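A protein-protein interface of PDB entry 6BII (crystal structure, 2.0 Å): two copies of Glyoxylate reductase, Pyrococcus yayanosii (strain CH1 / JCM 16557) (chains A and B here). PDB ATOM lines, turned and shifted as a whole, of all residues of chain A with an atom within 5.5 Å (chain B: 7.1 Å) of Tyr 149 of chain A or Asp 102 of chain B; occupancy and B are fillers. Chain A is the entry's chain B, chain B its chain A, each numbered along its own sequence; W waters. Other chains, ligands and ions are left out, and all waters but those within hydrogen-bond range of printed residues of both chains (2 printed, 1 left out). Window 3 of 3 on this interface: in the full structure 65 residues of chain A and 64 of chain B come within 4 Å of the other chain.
Of the 19 printed residues of chain B, 8 touch a printed residue of chain A. Hydrophobic or aromatic side chains of chain B within 4 Å of the printed part of chain A: Leu 107. Of the 10 printed residues of chain A, 6 touch a printed residue of chain B. Printed residues of chain A that touch a printed residue of chain B: Arg 117, Asp 147, Val 148, Tyr 149, Gly 171 and Phe 172. Along chain A the printed residues that touch a printed residue of chain B span positions 117 to 172. Among the printed residues, no Asp or Glu carboxylate lies within 4 Å of a Lys or Arg side-chain nitrogen of the other chain.
CB of Asp 106 of chain B touches NH1 of Arg 117 of chain A, 3.9 Å away. CB of Leu 107 of chain B touches NH2 of Arg 117 of chain A, 3.8 Å away. NH1 of Arg 117 of chain A touches CG2 of Thr 293 of chain B, 3.8 Å away. Asp 102 of chain B touches Tyr 149 of chain A (OD1 to CG, 3.8 Å). CD1 of Tyr 149 of chain A touches NH2 of Arg 168 of chain B (3.3 Å). Gly 171 of chain A touches Arg 168 of chain B. CE2 of Phe 172 of chain A touches OD1 of Asp 106 of chain B, at 3.4 Å. CZ of Phe 172 of chain A touches CG of Arg 168 of chain B, 3.6 Å away.
Water W2 lies within hydrogen-bond range of the side-chain carboxylate of Asp 106 of chain B, the guanidinium group of Arg 117 of chain A and the backbone NH of Val 148 of chain A. Water W1 bridges the side-chain hydroxyl (OH) of Tyr 149 of chain A (2.8 Å) and the side-chain amino group (NZ) of Lys 167 of chain B (2.9 Å).
The backbone carbonyl oxygen of Lys 167 of chain B sits close to the backbone carbonyl oxygen of Gly 171 of chain A, 3.4 Å away. O of Gly 290 of chain B is in hydrogen-bond range of NH2 of Arg 117 of chain A (2.9 Å). The backbone NH (N) of Val 148 of chain A lies within hydrogen-bond range of the side-chain carboxylate (OD2) of Asp 106 of chain B (3.1 Å). OD2 of Asp 106 of chain B is in hydrogen-bond range of N of Tyr 149 of chain A, 3.2 Å away. O of Ala 103 of chain B sits at hydrogen-bond distance from NH1 of Arg 117 of chain A (2.8 Å). OG1 of Thr 293 of chain B lies within hydrogen-bond range of OD1 of Asp 147 of chain A (2.9 Å).
No position is printed for both chains.
Tyr 149 of chain A touches three residues of chain B. Asp 102 of chain B touches just one residue of chain A: Tyr 149 (3.8 Å). Of the printed residues of chain A, Leu 107 of chain B touches Arg 117. Of the printed residues of chain B, Val 148 of chain A touches Asp 106. Printed residues of chain A within 4 Å of Gly 290 of chain B: Arg 117. Of the printed residues of chain A, Asp 106 of chain B touches Arg 117, Val 148, Tyr 149 and Phe 172. The nearest residue of chain A that does not touch Asp 102 of chain B is Arg 117 of chain A (5.1 Å).
The backbone NH (N) of Gly 150 of chain A sits at hydrogen-bond distance from the backbone carbonyl oxygen (O) of Phe 172 of chain A (2.9 Å). The side-chain carboxylate (OD1) of Asp 106 of chain B is in salt-bridge range of the guanidinium group (NE) of Arg 168 of chain B (2.9 Å). OD1 of Asp 102 of chain B is in salt-bridge range of NH2 of Arg 168 of chain B (2.9 Å). N of Thr 104 of chain B lies within hydrogen-bond range of O of Gly 290 of chain B (3.2 Å). The backbone carbonyl oxygen of Ala 164 of chain B sits at hydrogen-bond distance from the guanidinium group of Arg 168 of chain B (2.9 Å). The side-chain hydroxyl (OG1) of Thr 293 of chain B sits at hydrogen-bond distance from the backbone NH (N) of Ala 296 of chain B (3.1 Å).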
ATOM      1  N   ARG A 117      19.981   1.626  -5.874  1.00  0.00           N
ATOM      2  CA  ARG A 117      18.758   0.836  -5.727  1.00  0.00           C
ATOM      3  C   ARG A 117      18.252   0.646  -4.292  1.00  0.00           C
ATOM      4  O   ARG A 117      17.369  -0.153  -4.052  1.00  0.00           O
ATOM      5  CB  ARG A 117      18.937  -0.504  -6.460  1.00  0.00           C
ATOM      6  CG  ARG A 117      19.076  -0.365  -7.968  1.00  0.00           C
ATOM      7  CD  ARG A 117      17.849   0.285  -8.636  1.00  0.00           C
ATOM      8  NE  ARG A 117      16.687  -0.576  -8.463  1.00  0.00           N
ATOM      9  CZ  ARG A 117      16.417  -1.620  -9.236  1.00  0.00           C
ATOM     10  NH1 ARG A 117      17.140  -1.878 -10.326  1.00  0.00           N
ATOM     11  NH2 ARG A 117      15.379  -2.379  -8.975  1.00  0.00           N
ATOM     12  N   ASP A 147      17.965   3.530 -12.661  1.00  0.00           N
ATOM     13  CA  ASP A 147      18.519   2.625 -13.659  1.00  0.00           C
ATOM     14  C   ASP A 147      20.043   2.814 -13.752  1.00  0.00           C
ATOM     15  O   ASP A 147      20.547   3.933 -13.613  1.00  0.00           O
ATOM     16  CB  ASP A 147      17.884   2.896 -15.031  1.00  0.00           C
ATOM     17  CG  ASP A 147      16.463   2.394 -15.131  1.00  0.00           C
ATOM     18  OD1 ASP A 147      16.143   1.224 -14.774  1.00  0.00           O
ATOM     19  OD2 ASP A 147      15.664   3.215 -15.598  1.00  0.00           O
ATOM     20  N   VAL A 148      20.755   1.716 -13.971  1.00  0.00           N
ATOM     21  CA  VAL A 148      22.197   1.758 -14.207  1.00  0.00           C
ATOM     22  C   VAL A 148      22.551   1.352 -15.651  1.00  0.00           C
ATOM     23  O   VAL A 148      23.330   2.032 -16.321  1.00  0.00           O
ATOM     24  CB  VAL A 148      22.958   0.877 -13.192  1.00  0.00           C
ATOM     25  CG1 VAL A 148      24.468   0.914 -13.449  1.00  0.00           C
ATOM     26  CG2 VAL A 148      22.642   1.304 -11.780  1.00  0.00           C
ATOM     27  N   TYR A 149      21.991   0.244 -16.119  1.00  0.00           N
ATOM     28  CA  TYR A 149      22.280  -0.222 -17.473  1.00  0.00           C
ATOM     29  C   TYR A 149      22.048   0.879 -18.495  1.00  0.00           C
ATOM     30  O   TYR A 149      21.012   1.531 -18.483  1.00  0.00           O
ATOM     31  CB  TYR A 149      21.453  -1.453 -17.865  1.00  0.00           C
ATOM     32  CG  TYR A 149      22.028  -2.164 -19.059  1.00  0.00           C
ATOM     33  CD1 TYR A 149      22.996  -3.159 -18.890  1.00  0.00           C
ATOM     34  CD2 TYR A 149      21.646  -1.815 -20.368  1.00  0.00           C
ATOM     35  CE1 TYR A 149      23.550  -3.793 -19.994  1.00  0.00           C
ATOM     36  CE2 TYR A 149      22.222  -2.432 -21.489  1.00  0.00           C
ATOM     37  CZ  TYR A 149      23.187  -3.414 -21.278  1.00  0.00           C
ATOM     38  OH  TYR A 149      23.768  -4.052 -22.353  1.00  0.00           O
ATOM     39  N   GLY A 150      23.017   1.068 -19.382  1.00  0.00           N
ATOM     40  CA  GLY A 150      22.909   2.053 -20.472  1.00  0.00           C
ATOM     41  C   GLY A 150      23.127   3.514 -20.075  1.00  0.00           C
ATOM     42  O   GLY A 150      23.088   4.379 -20.910  1.00  0.00           O
ATOM     43  N   LYS A 151      23.306   3.812 -18.802  1.00  0.00           N
ATOM     44  CA  LYS A 151      23.525   5.184 -18.370  1.00  0.00           C
ATOM     45  C   LYS A 151      24.991   5.591 -18.541  1.00  0.00           C
ATOM     46  O   LYS A 151      25.810   4.830 -19.074  1.00  0.00           O
ATOM     47  CB  LYS A 151      23.075   5.304 -16.903  1.00  0.00           C
ATOM     48  CG  LYS A 151      21.597   5.011 -16.718  1.00  0.00           C
ATOM     49  CD  LYS A 151      20.764   6.119 -17.373  1.00  0.00           C
ATOM     50  CE  LYS A 151      19.321   5.819 -17.123  1.00  0.00           C
ATOM     51  NZ  LYS A 151      18.539   6.992 -17.541  1.00  0.00           N
ATOM     52  N   GLY A 171      30.046  -4.148 -19.139  1.00  0.00           N
ATOM     53  CA  GLY A 171      29.019  -5.170 -18.929  1.00  0.00           C
ATOM     54  C   GLY A 171      27.625  -4.591 -18.700  1.00  0.00           C
ATOM     55  O   GLY A 171      26.630  -5.210 -19.083  1.00  0.00           O
ATOM     56  N   PHE A 172      27.579  -3.380 -18.125  1.00  0.00           N
ATOM     57  CA  PHE A 172      26.351  -2.641 -17.967  1.00  0.00           C
ATOM     58  C   PHE A 172      25.997  -1.731 -19.158  1.00  0.00           C
ATOM     59  O   PHE A 172      25.109  -0.875 -19.043  1.00  0.00           O
ATOM     60  CB  PHE A 172      26.402  -1.871 -16.640  1.00  0.00           C
ATOM     61  CG  PHE A 172      26.146  -2.738 -15.427  1.00  0.00           C
ATOM     62  CD1 PHE A 172      27.131  -3.589 -14.948  1.00  0.00           C
ATOM     63  CD2 PHE A 172      24.896  -2.753 -14.807  1.00  0.00           C
ATOM     64  CE1 PHE A 172      26.901  -4.400 -13.854  1.00  0.00           C
ATOM     65  CE2 PHE A 172      24.659  -3.574 -13.729  1.00  0.00           C
ATOM     66  CZ  PHE A 172      25.664  -4.389 -13.238  1.00  0.00           C
ATOM     67  N   GLY A 173      26.630  -1.934 -20.308  1.00  0.00           N
ATOM     68  CA  GLY A 173      26.276  -1.183 -21.527  1.00  0.00           C
ATOM     69  C   GLY A 173      26.392   0.339 -21.415  1.00  0.00           C
ATOM     70  O   GLY A 173      25.699   1.066 -22.103  1.00  0.00           O
ATOM     71  N   MET A 174      27.280   0.825 -20.569  1.00  0.00           N
ATOM     72  CA  MET A 174      27.299   2.255 -20.229  1.00  0.00           C
ATOM     73  C   MET A 174      28.119   3.083 -21.207  1.00  0.00           C
ATOM     74  O   MET A 174      29.031   2.592 -21.850  1.00  0.00           O
ATOM     75  CB  MET A 174      27.865   2.432 -18.814  1.00  0.00           C
ATOM     76  CG  MET A 174      27.047   1.735 -17.740  1.00  0.00           C
ATOM     77  SD  MET A 174      27.593   2.037 -16.051  1.00  0.00           S
ATOM     78  CE  MET A 174      26.554   3.428 -15.639  1.00  0.00           C
ATOM     79  N   ASP B  98      10.317  -7.898 -20.828  1.00  0.00           N
ATOM     80  CA  ASP B  98      11.290  -7.026 -21.484  1.00  0.00           C
ATOM     81  C   ASP B  98      11.451  -5.639 -20.854  1.00  0.00           C
ATOM     82  O   ASP B  98      12.583  -5.213 -20.599  1.00  0.00           O
ATOM     83  CB  ASP B  98      11.027  -6.866 -22.977  1.00  0.00           C
ATOM     84  CG  ASP B  98      11.043  -8.193 -23.697  1.00  0.00           C
ATOM     85  OD1 ASP B  98      12.076  -8.905 -23.621  1.00  0.00           O
ATOM     86  OD2 ASP B  98      10.026  -8.533 -24.308  1.00  0.00           O
ATOM     87  N   VAL B  99      10.339  -4.947 -20.633  1.00  0.00           N
ATOM     88  CA  VAL B  99      10.351  -3.587 -20.094  1.00  0.00           C
ATOM     89  C   VAL B  99      10.970  -3.462 -18.697  1.00  0.00           C
ATOM     90  O   VAL B  99      11.383  -2.398 -18.306  1.00  0.00           O
ATOM     91  CB  VAL B  99       8.927  -2.961 -20.102  1.00  0.00           C
ATOM     92  CG1 VAL B  99       8.453  -2.776 -21.545  1.00  0.00           C
ATOM     93  CG2 VAL B  99       7.937  -3.803 -19.291  1.00  0.00           C
ATOM     94  N   LEU B 100      11.034  -4.562 -17.958  1.00  0.00           N
ATOM     95  CA  LEU B 100      11.560  -4.623 -16.601  1.00  0.00           C
ATOM     96  C   LEU B 100      12.865  -5.427 -16.484  1.00  0.00           C
ATOM     97  O   LEU B 100      13.369  -5.627 -15.401  1.00  0.00           O
ATOM     98  CB  LEU B 100      10.481  -5.189 -15.647  1.00  0.00           C
ATOM     99  CG  LEU B 100       9.719  -6.443 -16.084  1.00  0.00           C
ATOM    100  CD1 LEU B 100      10.626  -7.641 -16.375  1.00  0.00           C
ATOM    101  CD2 LEU B 100       8.693  -6.820 -15.027  1.00  0.00           C
ATOM    102  N   THR B 101      13.399  -5.889 -17.607  1.00  0.00           N
ATOM    103  CA  THR B 101      14.533  -6.794 -17.594  1.00  0.00           C
ATOM    104  C   THR B 101      15.758  -6.119 -16.984  1.00  0.00           C
ATOM    105  O   THR B 101      16.416  -6.689 -16.136  1.00  0.00           O
ATOM    106  CB  THR B 101      14.840  -7.275 -19.035  1.00  0.00           C
ATOM    107  OG1 THR B 101      13.769  -8.131 -19.473  1.00  0.00           O
ATOM    108  CG2 THR B 101      16.180  -7.978 -19.120  1.00  0.00           C
ATOM    109  N   ASP B 102      16.074  -4.918 -17.433  1.00  0.00           N
ATOM    110  CA  ASP B 102      17.281  -4.239 -16.976  1.00  0.00           C
ATOM    111  C   ASP B 102      17.218  -3.806 -15.521  1.00  0.00           C
ATOM    112  O   ASP B 102      18.219  -3.926 -14.824  1.00  0.00           O
ATOM    113  CB  ASP B 102      17.653  -3.069 -17.881  1.00  0.00           C
ATOM    114  CG  ASP B 102      18.248  -3.551 -19.195  1.00  0.00           C
ATOM    115  OD1 ASP B 102      19.012  -4.545 -19.242  1.00  0.00           O
ATOM    116  OD2 ASP B 102      17.942  -2.918 -20.183  1.00  0.00           O
ATOM    117  N   ALA B 103      16.052  -3.377 -15.057  1.00  0.00           N
ATOM    118  CA  ALA B 103      15.899  -3.075 -13.632  1.00  0.00           C
ATOM    119  C   ALA B 103      16.140  -4.325 -12.781  1.00  0.00           C
ATOM    120  O   ALA B 103      16.902  -4.283 -11.806  1.00  0.00           O
ATOM    121  CB  ALA B 103      14.532  -2.471 -13.331  1.00  0.00           C
ATOM    122  N   THR B 104      15.537  -5.438 -13.160  1.00  0.00           N
ATOM    123  CA  THR B 104      15.662  -6.664 -12.368  1.00  0.00           C
ATOM    124  C   THR B 104      17.090  -7.235 -12.370  1.00  0.00           C
ATOM    125  O   THR B 104      17.598  -7.670 -11.334  1.00  0.00           O
ATOM    126  CB  THR B 104      14.639  -7.730 -12.809  1.00  0.00           C
ATOM    127  OG1 THR B 104      13.325  -7.157 -12.796  1.00  0.00           O
ATOM    128  CG2 THR B 104      14.663  -8.923 -11.858  1.00  0.00           C
ATOM    129  N   ALA B 105      17.711  -7.268 -13.540  1.00  0.00           N
ATOM    130  CA  ALA B 105      19.106  -7.708 -13.645  1.00  0.00           C
ATOM    131  C   ALA B 105      20.086  -6.796 -12.887  1.00  0.00           C
ATOM    132  O   ALA B 105      21.039  -7.300 -12.286  1.00  0.00           O
ATOM    133  CB  ALA B 105      19.528  -7.819 -15.109  1.00  0.00           C
ATOM    134  N   ASP B 106      19.869  -5.476 -12.927  1.00  0.00           N
ATOM    135  CA  ASP B 106      20.667  -4.549 -12.103  1.00  0.00           C
ATOM    136  C   ASP B 106      20.517  -4.896 -10.611  1.00  0.00           C
ATOM    137  O   ASP B 106      21.497  -4.931  -9.877  1.00  0.00           O
ATOM    138  CB  ASP B 106      20.249  -3.092 -12.296  1.00  0.00           C
ATOM    139  CG  ASP B 106      20.662  -2.492 -13.654  1.00  0.00           C
ATOM    140  OD1 ASP B 106      21.363  -3.159 -14.469  1.00  0.00           O
ATOM    141  OD2 ASP B 106      20.275  -1.312 -13.871  1.00  0.00           O
ATOM    142  N   LEU B 107      19.288  -5.144 -10.173  1.00  0.00           N
ATOM    143  CA  LEU B 107      19.050  -5.464  -8.761  1.00  0.00           C
ATOM    144  C   LEU B 107      19.729  -6.799  -8.368  1.00  0.00           C
ATOM    145  O   LEU B 107      20.318  -6.906  -7.281  1.00  0.00           O
ATOM    146  CB  LEU B 107      17.553  -5.458  -8.387  1.00  0.00           C
ATOM    147  CG  LEU B 107      17.512  -5.683  -6.877  1.00  0.00           C
ATOM    148  CD1 LEU B 107      17.787  -4.397  -6.127  1.00  0.00           C
ATOM    149  CD2 LEU B 107      16.301  -6.400  -6.393  1.00  0.00           C
ATOM    150  N   ALA B 108      19.693  -7.794  -9.258  1.00  0.00           N
ATOM    151  CA  ALA B 108      20.363  -9.062  -8.989  1.00  0.00           C
ATOM    152  C   ALA B 108      21.846  -8.845  -8.751  1.00  0.00           C
ATOM    153  O   ALA B 108      22.423  -9.427  -7.837  1.00  0.00           O
ATOM    154  CB  ALA B 108      20.163 -10.060 -10.137  1.00  0.00           C
ATOM    155  N   ARG B 160      15.006 -13.898 -20.533  1.00  0.00           N
ATOM    156  CA  ARG B 160      15.267 -12.465 -20.670  1.00  0.00           C
ATOM    157  C   ARG B 160      16.127 -11.939 -19.503  1.00  0.00           C
ATOM    158  O   ARG B 160      17.163 -11.301 -19.733  1.00  0.00           O
ATOM    159  CB  ARG B 160      13.937 -11.728 -20.755  1.00  0.00           C
ATOM    160  CG  ARG B 160      13.115 -12.064 -22.022  1.00  0.00           C
ATOM    161  CD  ARG B 160      11.674 -11.568 -21.894  1.00  0.00           C
ATOM    162  NE  ARG B 160      10.885 -12.336 -20.901  1.00  0.00           N
ATOM    163  CZ  ARG B 160       9.806 -13.075 -21.171  1.00  0.00           C
ATOM    164  NH1 ARG B 160       9.325 -13.168 -22.430  1.00  0.00           N
ATOM    165  NH2 ARG B 160       9.169 -13.712 -20.187  1.00  0.00           N
ATOM    166  N   ILE B 161      15.737 -12.268 -18.271  1.00  0.00           N
ATOM    167  CA  ILE B 161      16.433 -11.743 -17.102  1.00  0.00           C
ATOM    168  C   ILE B 161      17.761 -12.469 -16.881  1.00  0.00           C
ATOM    169  O   ILE B 161      18.795 -11.839 -16.647  1.00  0.00           O
ATOM    170  CB  ILE B 161      15.523 -11.737 -15.867  1.00  0.00           C
ATOM    171  CG1 ILE B 161      14.383 -10.718 -16.082  1.00  0.00           C
ATOM    172  CG2 ILE B 161      16.332 -11.387 -14.627  1.00  0.00           C
ATOM    173  CD1 ILE B 161      13.224 -10.866 -15.132  1.00  0.00           C
ATOM    174  N   ALA B 164      20.317 -11.215 -19.330  1.00  0.00           N
ATOM    175  CA  ALA B 164      20.766  -9.866 -18.901  1.00  0.00           C
ATOM    176  C   ALA B 164      21.776  -9.916 -17.748  1.00  0.00           C
ATOM    177  O   ALA B 164      22.751  -9.153 -17.716  1.00  0.00           O
ATOM    178  CB  ALA B 164      19.573  -9.014 -18.531  1.00  0.00           C
ATOM    179  N   LYS B 167      25.040 -10.751 -19.361  1.00  0.00           N
ATOM    180  CA  LYS B 167      25.689  -9.595 -20.031  1.00  0.00           C
ATOM    181  C   LYS B 167      26.512  -8.797 -19.008  1.00  0.00           C
ATOM    182  O   LYS B 167      27.637  -8.430 -19.267  1.00  0.00           O
ATOM    183  CB  LYS B 167      24.677  -8.640 -20.656  1.00  0.00           C
ATOM    184  CG  LYS B 167      23.987  -9.190 -21.860  1.00  0.00           C
ATOM    185  CD  LYS B 167      23.003  -8.208 -22.482  1.00  0.00           C
ATOM    186  CE  LYS B 167      22.143  -8.969 -23.495  1.00  0.00           C
ATOM    187  NZ  LYS B 167      21.263  -8.065 -24.279  1.00  0.00           N
ATOM    188  N   ARG B 168      25.931  -8.553 -17.844  1.00  0.00           N
ATOM    189  CA  ARG B 168      26.657  -7.842 -16.786  1.00  0.00           C
ATOM    190  C   ARG B 168      27.885  -8.654 -16.307  1.00  0.00           C
ATOM    191  O   ARG B 168      28.978  -8.083 -16.121  1.00  0.00           O
ATOM    192  CB  ARG B 168      25.698  -7.487 -15.656  1.00  0.00           C
ATOM    193  CG  ARG B 168      24.669  -6.411 -16.062  1.00  0.00           C
ATOM    194  CD  ARG B 168      23.368  -6.587 -15.316  1.00  0.00           C
ATOM    195  NE  ARG B 168      22.341  -5.599 -15.644  1.00  0.00           N
ATOM    196  CZ  ARG B 168      21.652  -5.538 -16.774  1.00  0.00           C
ATOM    197  NH1 ARG B 168      21.858  -6.404 -17.768  1.00  0.00           N
ATOM    198  NH2 ARG B 168      20.742  -4.602 -16.905  1.00  0.00           N
ATOM    199  N   GLY B 290      12.863  -5.802  -7.341  1.00  0.00           N
ATOM    200  CA  GLY B 290      13.526  -6.072  -8.602  1.00  0.00           C
ATOM    201  C   GLY B 290      13.225  -5.089  -9.739  1.00  0.00           C
ATOM    202  O   GLY B 290      14.157  -4.587 -10.380  1.00  0.00           O
ATOM    203  N   THR B 293      12.326   0.677 -10.731  1.00  0.00           N
ATOM    204  CA  THR B 293      12.775   1.952 -11.288  1.00  0.00           C
ATOM    205  C   THR B 293      11.587   2.565 -12.007  1.00  0.00           C
ATOM    206  O   THR B 293      10.695   1.850 -12.533  1.00  0.00           O
ATOM    207  CB  THR B 293      13.959   1.835 -12.278  1.00  0.00           C
ATOM    208  OG1 THR B 293      13.534   1.196 -13.496  1.00  0.00           O
ATOM    209  CG2 THR B 293      15.141   1.088 -11.630  1.00  0.00           C
ATOM    210  N   ALA B 296      11.200   1.187 -15.601  1.00  0.00           N
ATOM    211  CA  ALA B 296      10.581  -0.132 -15.678  1.00  0.00           C
ATOM    212  C   ALA B 296       9.072  -0.095 -15.422  1.00  0.00           C
ATOM    213  O   ALA B 296       8.281  -0.651 -16.183  1.00  0.00           O
ATOM    214  CB  ALA B 296      11.265  -1.120 -14.748  1.00  0.00           C
HETATM  215  O   HOH W   1      21.439  -5.405 -23.098  1.00  0.00           O
HETATM  216  O   HOH W   2      19.076  -0.175 -11.644  1.00  0.00           O
